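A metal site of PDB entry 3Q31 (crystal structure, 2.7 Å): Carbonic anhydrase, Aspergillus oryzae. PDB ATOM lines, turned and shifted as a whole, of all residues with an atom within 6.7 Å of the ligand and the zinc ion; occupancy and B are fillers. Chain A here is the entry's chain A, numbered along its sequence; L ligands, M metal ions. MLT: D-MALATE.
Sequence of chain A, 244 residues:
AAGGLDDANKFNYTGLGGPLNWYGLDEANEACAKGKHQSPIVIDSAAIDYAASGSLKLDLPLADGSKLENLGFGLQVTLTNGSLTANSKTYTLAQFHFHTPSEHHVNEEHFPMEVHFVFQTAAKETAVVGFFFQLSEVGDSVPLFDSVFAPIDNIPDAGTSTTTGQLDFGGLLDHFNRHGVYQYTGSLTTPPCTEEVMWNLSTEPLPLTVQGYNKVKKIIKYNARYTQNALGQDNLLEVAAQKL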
ATOM      1  N   PHE A  11      18.530  -9.583  11.449  1.00  0.00           N
ATOM      2  CA  PHE A  11      18.842  -8.639  12.504  1.00  0.00           C
ATOM      3  C   PHE A  11      20.102  -7.814  12.148  1.00  0.00           C
ATOM      4  O   PHE A  11      21.193  -8.064  12.665  1.00  0.00           O
ATOM      5  CB  PHE A  11      18.960  -9.350  13.856  1.00  0.00           C
ATOM      6  CG  PHE A  11      19.395  -8.451  14.995  1.00  0.00           C
ATOM      7  CD1 PHE A  11      19.916  -8.986  16.150  1.00  0.00           C
ATOM      8  CD2 PHE A  11      19.291  -7.080  14.888  1.00  0.00           C
ATOM      9  CE1 PHE A  11      20.325  -8.176  17.178  1.00  0.00           C
ATOM     10  CE2 PHE A  11      19.721  -6.276  15.921  1.00  0.00           C
ATOM     11  CZ  PHE A  11      20.233  -6.823  17.059  1.00  0.00           C
ATOM     12  N   TYR A  13      21.428  -3.604  10.615  1.00  0.00           N
ATOM     13  CA  TYR A  13      21.298  -2.149  10.812  1.00  0.00           C
ATOM     14  C   TYR A  13      21.069  -1.449   9.487  1.00  0.00           C
ATOM     15  O   TYR A  13      20.765  -0.260   9.410  1.00  0.00           O
ATOM     16  CB  TYR A  13      22.513  -1.566  11.534  1.00  0.00           C
ATOM     17  CG  TYR A  13      22.498  -1.856  13.019  1.00  0.00           C
ATOM     18  CD1 TYR A  13      21.845  -1.011  13.906  1.00  0.00           C
ATOM     19  CD2 TYR A  13      23.126  -2.980  13.526  1.00  0.00           C
ATOM     20  CE1 TYR A  13      21.810  -1.284  15.258  1.00  0.00           C
ATOM     21  CE2 TYR A  13      23.101  -3.258  14.870  1.00  0.00           C
ATOM     22  CZ  TYR A  13      22.449  -2.416  15.734  1.00  0.00           C
ATOM     23  OH  TYR A  13      22.445  -2.715  17.081  1.00  0.00           O
ATOM     24  N   LEU A  71      30.170 -10.562  16.968  1.00  0.00           N
ATOM     25  CA  LEU A  71      28.752 -10.785  16.707  1.00  0.00           C
ATOM     26  C   LEU A  71      28.343 -10.617  15.249  1.00  0.00           C
ATOM     27  O   LEU A  71      27.311 -11.119  14.831  1.00  0.00           O
ATOM     28  CB  LEU A  71      27.912  -9.809  17.533  1.00  0.00           C
ATOM     29  CG  LEU A  71      27.883 -10.025  19.040  1.00  0.00           C
ATOM     30  CD1 LEU A  71      26.827  -9.093  19.621  1.00  0.00           C
ATOM     31  CD2 LEU A  71      27.589 -11.481  19.356  1.00  0.00           C
ATOM     32  N   GLN A  76      31.209  -8.346  21.661  1.00  0.00           N
ATOM     33  CA  GLN A  76      30.687  -8.689  22.979  1.00  0.00           C
ATOM     34  C   GLN A  76      31.612  -9.602  23.778  1.00  0.00           C
ATOM     35  O   GLN A  76      32.170 -10.599  23.280  1.00  0.00           O
ATOM     36  CB  GLN A  76      29.332  -9.360  22.817  1.00  0.00           C
ATOM     37  CG  GLN A  76      28.683  -9.747  24.098  1.00  0.00           C
ATOM     38  CD  GLN A  76      27.235 -10.167  23.920  1.00  0.00           C
ATOM     39  OE1 GLN A  76      26.580  -9.777  22.954  1.00  0.00           O
ATOM     40  NE2 GLN A  76      26.741 -10.975  24.853  1.00  0.00           N
ATOM     41  N   GLN A  95      26.829 -10.181  30.280  1.00  0.00           N
ATOM     42  CA  GLN A  95      27.809  -9.822  29.237  1.00  0.00           C
ATOM     43  C   GLN A  95      27.939  -8.311  29.106  1.00  0.00           C
ATOM     44  O   GLN A  95      27.054  -7.562  29.528  1.00  0.00           O
ATOM     45  CB  GLN A  95      27.399 -10.396  27.881  1.00  0.00           C
ATOM     46  CG  GLN A  95      25.907 -10.176  27.511  1.00  0.00           C
ATOM     47  CD  GLN A  95      25.632  -8.875  26.756  1.00  0.00           C
ATOM     48  OE1 GLN A  95      26.542  -8.220  26.247  1.00  0.00           O
ATOM     49  NE2 GLN A  95      24.361  -8.497  26.676  1.00  0.00           N
ATOM     50  N   HIS A  97      29.095  -5.198  26.012  1.00  0.00           N
ATOM     51  CA  HIS A  97      29.377  -5.035  24.588  1.00  0.00           C
ATOM     52  C   HIS A  97      29.421  -3.568  24.146  1.00  0.00           C
ATOM     53  O   HIS A  97      29.144  -2.632  24.927  1.00  0.00           O
ATOM     54  CB  HIS A  97      28.352  -5.805  23.772  1.00  0.00           C
ATOM     55  CG  HIS A  97      26.969  -5.246  23.878  1.00  0.00           C
ATOM     56  ND1 HIS A  97      26.190  -5.421  24.999  1.00  0.00           N
ATOM     57  CD2 HIS A  97      26.244  -4.493  23.026  1.00  0.00           C
ATOM     58  CE1 HIS A  97      25.026  -4.810  24.826  1.00  0.00           C
ATOM     59  NE2 HIS A  97      25.034  -4.238  23.634  1.00  0.00           N
ATOM     60  N   PHE A  98      29.770  -3.367  22.880  1.00  0.00           N
ATOM     61  CA  PHE A  98      30.082  -2.039  22.410  1.00  0.00           C
ATOM     62  C   PHE A  98      29.247  -1.626  21.239  1.00  0.00           C
ATOM     63  O   PHE A  98      28.857  -2.454  20.417  1.00  0.00           O
ATOM     64  CB  PHE A  98      31.552  -1.948  22.062  1.00  0.00           C
ATOM     65  CG  PHE A  98      32.427  -2.356  23.183  1.00  0.00           C
ATOM     66  CD1 PHE A  98      32.698  -3.695  23.397  1.00  0.00           C
ATOM     67  CD2 PHE A  98      32.931  -1.416  24.056  1.00  0.00           C
ATOM     68  CE1 PHE A  98      33.482  -4.078  24.436  1.00  0.00           C
ATOM     69  CE2 PHE A  98      33.726  -1.815  25.107  1.00  0.00           C
ATOM     70  CZ  PHE A  98      33.986  -3.144  25.301  1.00  0.00           C
ATOM     71  N   HIS A  99      28.967  -0.334  21.189  1.00  0.00           N
ATOM     72  CA  HIS A  99      28.290   0.294  20.075  1.00  0.00           C
ATOM     73  C   HIS A  99      29.122   1.455  19.570  1.00  0.00           C
ATOM     74  O   HIS A  99      29.726   2.225  20.345  1.00  0.00           O
ATOM     75  CB  HIS A  99      26.964   0.860  20.528  1.00  0.00           C
ATOM     76  CG  HIS A  99      25.956  -0.172  20.914  1.00  0.00           C
ATOM     77  ND1 HIS A  99      25.144  -0.788  19.990  1.00  0.00           N
ATOM     78  CD2 HIS A  99      25.602  -0.652  22.126  1.00  0.00           C
ATOM     79  CE1 HIS A  99      24.333  -1.620  20.623  1.00  0.00           C
ATOM     80  NE2 HIS A  99      24.601  -1.559  21.909  1.00  0.00           N
ATOM     81  N   GLU A 103      24.764   5.176  21.195  1.00  0.00           N
ATOM     82  CA  GLU A 103      23.360   5.065  20.847  1.00  0.00           C
ATOM     83  C   GLU A 103      22.623   6.212  21.490  1.00  0.00           C
ATOM     84  O   GLU A 103      21.811   6.870  20.843  1.00  0.00           O
ATOM     85  CB  GLU A 103      22.788   3.728  21.287  1.00  0.00           C
ATOM     86  CG  GLU A 103      23.499   2.519  20.697  1.00  0.00           C
ATOM     87  CD  GLU A 103      22.603   1.317  20.610  1.00  0.00           C
ATOM     88  OE1 GLU A 103      22.527   0.544  21.598  1.00  0.00           O
ATOM     89  OE2 GLU A 103      21.959   1.147  19.563  1.00  0.00           O
ATOM     90  N   GLU A 114      29.923   3.629  22.822  1.00  0.00           N
ATOM     91  CA  GLU A 114      29.179   3.343  24.044  1.00  0.00           C
ATOM     92  C   GLU A 114      29.365   1.886  24.466  1.00  0.00           C
ATOM     93  O   GLU A 114      29.278   1.001  23.609  1.00  0.00           O
ATOM     94  CB  GLU A 114      27.701   3.659  23.815  1.00  0.00           C
ATOM     95  CG  GLU A 114      26.850   3.672  25.059  1.00  0.00           C
ATOM     96  CD  GLU A 114      25.469   4.258  24.811  1.00  0.00           C
ATOM     97  OE1 GLU A 114      25.290   5.085  23.884  1.00  0.00           O
ATOM     98  OE2 GLU A 114      24.541   3.906  25.574  1.00  0.00           O
ATOM     99  N   VAL A 115      29.630   1.626  25.761  1.00  0.00           N
ATOM    100  CA  VAL A 115      29.599   0.258  26.331  1.00  0.00           C
ATOM    101  C   VAL A 115      28.347  -0.033  27.136  1.00  0.00           C
ATOM    102  O   VAL A 115      27.876   0.799  27.918  1.00  0.00           O
ATOM    103  CB  VAL A 115      30.689  -0.028  27.366  1.00  0.00           C
ATOM    104  CG1 VAL A 115      31.452  -1.316  27.012  1.00  0.00           C
ATOM    105  CG2 VAL A 115      31.585   1.158  27.573  1.00  0.00           C
ATOM    106  N   HIS A 116      27.864  -1.262  26.977  1.00  0.00           N
ATOM    107  CA  HIS A 116      26.692  -1.719  27.692  1.00  0.00           C
ATOM    108  C   HIS A 116      27.031  -2.921  28.552  1.00  0.00           C
ATOM    109  O   HIS A 116      27.481  -3.958  28.039  1.00  0.00           O
ATOM    110  CB  HIS A 116      25.598  -2.100  26.706  1.00  0.00           C
ATOM    111  CG  HIS A 116      24.957  -0.905  26.055  1.00  0.00           C
ATOM    112  ND1 HIS A 116      24.269  -0.990  24.852  1.00  0.00           N
ATOM    113  CD2 HIS A 116      24.885   0.388  26.437  1.00  0.00           C
ATOM    114  CE1 HIS A 116      23.806   0.209  24.532  1.00  0.00           C
ATOM    115  NE2 HIS A 116      24.164   1.055  25.474  1.00  0.00           N
ATOM    116  N   PHE A 117      26.864  -2.782  29.862  1.00  0.00           N
ATOM    117  CA  PHE A 117      26.989  -3.928  30.747  1.00  0.00           C
ATOM    118  C   PHE A 117      25.579  -4.375  31.047  1.00  0.00           C
ATOM    119  O   PHE A 117      24.772  -3.594  31.583  1.00  0.00           O
ATOM    120  CB  PHE A 117      27.691  -3.551  32.043  1.00  0.00           C
ATOM    121  CG  PHE A 117      29.174  -3.369  31.901  1.00  0.00           C
ATOM    122  CD1 PHE A 117      29.710  -2.127  31.607  1.00  0.00           C
ATOM    123  CD2 PHE A 117      30.032  -4.446  32.048  1.00  0.00           C
ATOM    124  CE1 PHE A 117      31.084  -1.962  31.484  1.00  0.00           C
ATOM    125  CE2 PHE A 117      31.407  -4.295  31.922  1.00  0.00           C
ATOM    126  CZ  PHE A 117      31.933  -3.049  31.637  1.00  0.00           C
ATOM    127  N   VAL A 118      25.268  -5.610  30.671  1.00  0.00           N
ATOM    128  CA  VAL A 118      23.913  -6.122  30.799  1.00  0.00           C
ATOM    129  C   VAL A 118      23.756  -7.088  31.973  1.00  0.00           C
ATOM    130  O   VAL A 118      24.442  -8.117  32.044  1.00  0.00           O
ATOM    131  CB  VAL A 118      23.459  -6.828  29.518  1.00  0.00           C
ATOM    132  CG1 VAL A 118      22.005  -7.175  29.628  1.00  0.00           C
ATOM    133  CG2 VAL A 118      23.690  -5.941  28.328  1.00  0.00           C
ATOM    134  N   THR A 126      15.707  -6.800  33.576  1.00  0.00           N
ATOM    135  CA  THR A 126      17.028  -6.356  33.118  1.00  0.00           C
ATOM    136  C   THR A 126      17.401  -4.966  33.610  1.00  0.00           C
ATOM    137  O   THR A 126      16.532  -4.110  33.816  1.00  0.00           O
ATOM    138  CB  THR A 126      17.096  -6.302  31.601  1.00  0.00           C
ATOM    139  OG1 THR A 126      16.769  -7.592  31.055  1.00  0.00           O
ATOM    140  CG2 THR A 126      18.498  -5.856  31.157  1.00  0.00           C
ATOM    141  N   ALA A 127      18.699  -4.743  33.793  1.00  0.00           N
ATOM    142  CA  ALA A 127      19.247  -3.417  34.071  1.00  0.00           C
ATOM    143  C   ALA A 127      20.527  -3.278  33.273  1.00  0.00           C
ATOM    144  O   ALA A 127      21.223  -4.266  33.028  1.00  0.00           O
ATOM    145  CB  ALA A 127      19.537  -3.236  35.553  1.00  0.00           C
ATOM    146  N   VAL A 128      20.854  -2.046  32.856  1.00  0.00           N
ATOM    147  CA  VAL A 128      22.098  -1.810  32.148  1.00  0.00           C
ATOM    148  C   VAL A 128      22.968  -0.771  32.838  1.00  0.00           C
ATOM    149  O   VAL A 128      22.480   0.225  33.401  1.00  0.00           O
ATOM    150  CB  VAL A 128      21.861  -1.319  30.710  1.00  0.00           C
ATOM    151  CG1 VAL A 128      23.196  -1.084  30.031  1.00  0.00           C
ATOM    152  CG2 VAL A 128      21.028  -2.293  29.918  1.00  0.00           C
ATOM    153  N   SER A 187      14.267   0.500  27.286  1.00  0.00           N
ATOM    154  CA  SER A 187      14.170  -0.781  26.612  1.00  0.00           C
ATOM    155  C   SER A 187      15.523  -1.291  26.134  1.00  0.00           C
ATOM    156  O   SER A 187      16.548  -0.632  26.302  1.00  0.00           O
ATOM    157  CB  SER A 187      13.281  -0.649  25.387  1.00  0.00           C
ATOM    158  OG  SER A 187      14.079  -0.267  24.285  1.00  0.00           O
ATOM    159  N   LEU A 188      15.491  -2.473  25.529  1.00  0.00           N
ATOM    160  CA  LEU A 188      16.647  -3.020  24.850  1.00  0.00           C
ATOM    161  C   LEU A 188      16.816  -2.268  23.555  1.00  0.00           C
ATOM    162  O   LEU A 188      15.820  -1.911  22.922  1.00  0.00           O
ATOM    163  CB  LEU A 188      16.388  -4.472  24.489  1.00  0.00           C
ATOM    164  CG  LEU A 188      16.201  -5.431  25.657  1.00  0.00           C
ATOM    165  CD1 LEU A 188      16.362  -6.864  25.133  1.00  0.00           C
ATOM    166  CD2 LEU A 188      17.227  -5.107  26.725  1.00  0.00           C
ATOM    167  N   THR A 189      18.048  -2.034  23.150  1.00  0.00           N
ATOM    168  CA  THR A 189      18.289  -1.317  21.905  1.00  0.00           C
ATOM    169  C   THR A 189      18.440  -2.295  20.749  1.00  0.00           C
ATOM    170  O   THR A 189      18.839  -1.929  19.652  1.00  0.00           O
ATOM    171  CB  THR A 189      19.491  -0.410  21.999  1.00  0.00           C
ATOM    172  OG1 THR A 189      20.664  -1.198  22.266  1.00  0.00           O
ATOM    173  CG2 THR A 189      19.290   0.577  23.135  1.00  0.00           C
ATOM    174  N   THR A 190      18.106  -3.556  21.016  1.00  0.00           N
ATOM    175  CA  THR A 190      18.098  -4.567  19.984  1.00  0.00           C
ATOM    176  C   THR A 190      16.807  -5.358  20.122  1.00  0.00           C
ATOM    177  O   THR A 190      16.177  -5.331  21.174  1.00  0.00           O
ATOM    178  CB  THR A 190      19.340  -5.508  20.056  1.00  0.00           C
ATOM    179  OG1 THR A 190      19.564  -5.945  21.396  1.00  0.00           O
ATOM    180  CG2 THR A 190      20.576  -4.777  19.582  1.00  0.00           C
ATOM    181  N   PRO A 191      16.411  -6.046  19.060  1.00  0.00           N
ATOM    182  CA  PRO A 191      15.161  -6.816  19.102  1.00  0.00           C
ATOM    183  C   PRO A 191      15.261  -7.894  20.181  1.00  0.00           C
ATOM    184  O   PRO A 191      16.298  -8.560  20.300  1.00  0.00           O
ATOM    185  CB  PRO A 191      15.106  -7.465  17.715  1.00  0.00           C
ATOM    186  CG  PRO A 191      16.102  -6.697  16.867  1.00  0.00           C
ATOM    187  CD  PRO A 191      17.153  -6.268  17.819  1.00  0.00           C
ATOM    188  N   VAL A 197      13.528  -1.892  30.951  1.00  0.00           N
ATOM    189  CA  VAL A 197      14.953  -1.978  31.239  1.00  0.00           C
ATOM    190  C   VAL A 197      15.375  -0.831  32.138  1.00  0.00           C
ATOM    191  O   VAL A 197      14.935   0.297  31.963  1.00  0.00           O
ATOM    192  CB  VAL A 197      15.800  -1.914  29.966  1.00  0.00           C
ATOM    193  CG1 VAL A 197      17.295  -1.829  30.324  1.00  0.00           C
ATOM    194  CG2 VAL A 197      15.491  -3.127  29.069  1.00  0.00           C
ATOM    195  N   TRP A 199      17.907   1.696  32.996  1.00  0.00           N
ATOM    196  CA  TRP A 199      19.060   2.299  32.375  1.00  0.00           C
ATOM    197  C   TRP A 199      19.859   3.142  33.350  1.00  0.00           C
ATOM    198  O   TRP A 199      19.326   4.033  34.030  1.00  0.00           O
ATOM    199  CB  TRP A 199      18.645   3.109  31.136  1.00  0.00           C
ATOM    200  CG  TRP A 199      18.569   2.276  29.908  1.00  0.00           C
ATOM    201  CD1 TRP A 199      17.463   1.684  29.379  1.00  0.00           C
ATOM    202  CD2 TRP A 199      19.665   1.934  29.053  1.00  0.00           C
ATOM    203  NE1 TRP A 199      17.788   0.995  28.228  1.00  0.00           N
ATOM    204  CE2 TRP A 199      19.135   1.128  28.004  1.00  0.00           C
ATOM    205  CE3 TRP A 199      21.030   2.241  29.050  1.00  0.00           C
ATOM    206  CZ2 TRP A 199      19.931   0.612  26.987  1.00  0.00           C
ATOM    207  CZ3 TRP A 199      21.827   1.720  28.024  1.00  0.00           C
ATOM    208  CH2 TRP A 199      21.267   0.912  27.012  1.00  0.00           C
HETATM  209  C1  MLT L   1      21.490  -6.341  23.978  1.00  0.00           C
HETATM  210  O1  MLT L   1      22.499  -7.058  24.131  1.00  0.00           O
HETATM  211  O2  MLT L   1      20.368  -6.893  23.939  1.00  0.00           O
HETATM  212  C2  MLT L   1      21.609  -4.835  23.875  1.00  0.00           C
HETATM  213  O3  MLT L   1      21.661  -4.314  22.550  1.00  0.00           O
HETATM  214  C3  MLT L   1      20.610  -4.057  24.707  1.00  0.00           C
HETATM  215  C4  MLT L   1      21.541  -3.228  25.528  1.00  0.00           C
HETATM  216  O4  MLT L   1      21.151  -2.643  26.565  1.00  0.00           O
HETATM  217  O5  MLT L   1      22.751  -3.156  25.170  1.00  0.00           O
HETATM  218 ZN    ZN M   1      23.803  -2.574  23.558  1.00  0.00          ZN
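An oxygen (O2) of the ligand sits at hydrogen-bond distance from the side-chain hydroxyl (OG1) of Thr 190, 2.8 Å away. OG1 of Thr 189 lies within hydrogen-bond range of O3 of the ligand (3.3 Å). An oxygen (O1) of the ligand sits at hydrogen-bond distance from the side-chain amide nitrogen (NE2) of Gln 95 (3.5 Å).
The side-chain carboxylate (OE1) of Glu 103 sits close to a ring nitrogen (ND1) of His 99, 3.3 Å away. N of His 99 is in hydrogen-bond range of O of Glu 114. A ring nitrogen (NE2) of His 116 is in hydrogen-bond range of the side-chain carboxylate of Glu 114 (2.9 Å). OE1 of Glu 103 is in hydrogen-bond range of OG1 of Thr 189 (2.6 Å). N of Val 118 sits at hydrogen-bond distance from O of Gln 95. NE2 of Gln 76 lies close to OE1 of Gln 95, at 3.1 Å. The indole nitrogen (NE1) of Trp 199 is in hydrogen-bond range of the backbone carbonyl oxygen (O) of Ser 187 (2.8 Å). The backbone NH (N) of Glu 103 sits at hydrogen-bond distance from the side-chain carboxylate (OE1) of Glu 114 (2.7 Å).
CG2 of Val 128 touches O4 of the ligand (3.4 Å). Trp 199 touches the ligand (CZ2 to O4, 3.5 Å). Hydrophobic or aromatic side chains that line the ligand: His 97, His 116, Val 128 and Trp 199. Within 4 Å of the ligand: Gln 95, His 97, His 116, Val 128, Thr 189, Thr 190 and Trp 199. Along chain A the residues within 4 Å of the ligand span positions 95 to 199.
Merely in contact with the zinc ion: Glu 103 and Thr 189. The nearest printed residue that does not touch the zinc ion is Trp 199 (5.5 Å).
The zinc ion is bound by O5 of the ligand (2.0 Å), NE2 of His 97 (2.1 Å), NE2 of His 99 (2.1 Å) and ND1 of His 116 (2.1 Å). The zinc ion has four donor atoms within binding distance.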
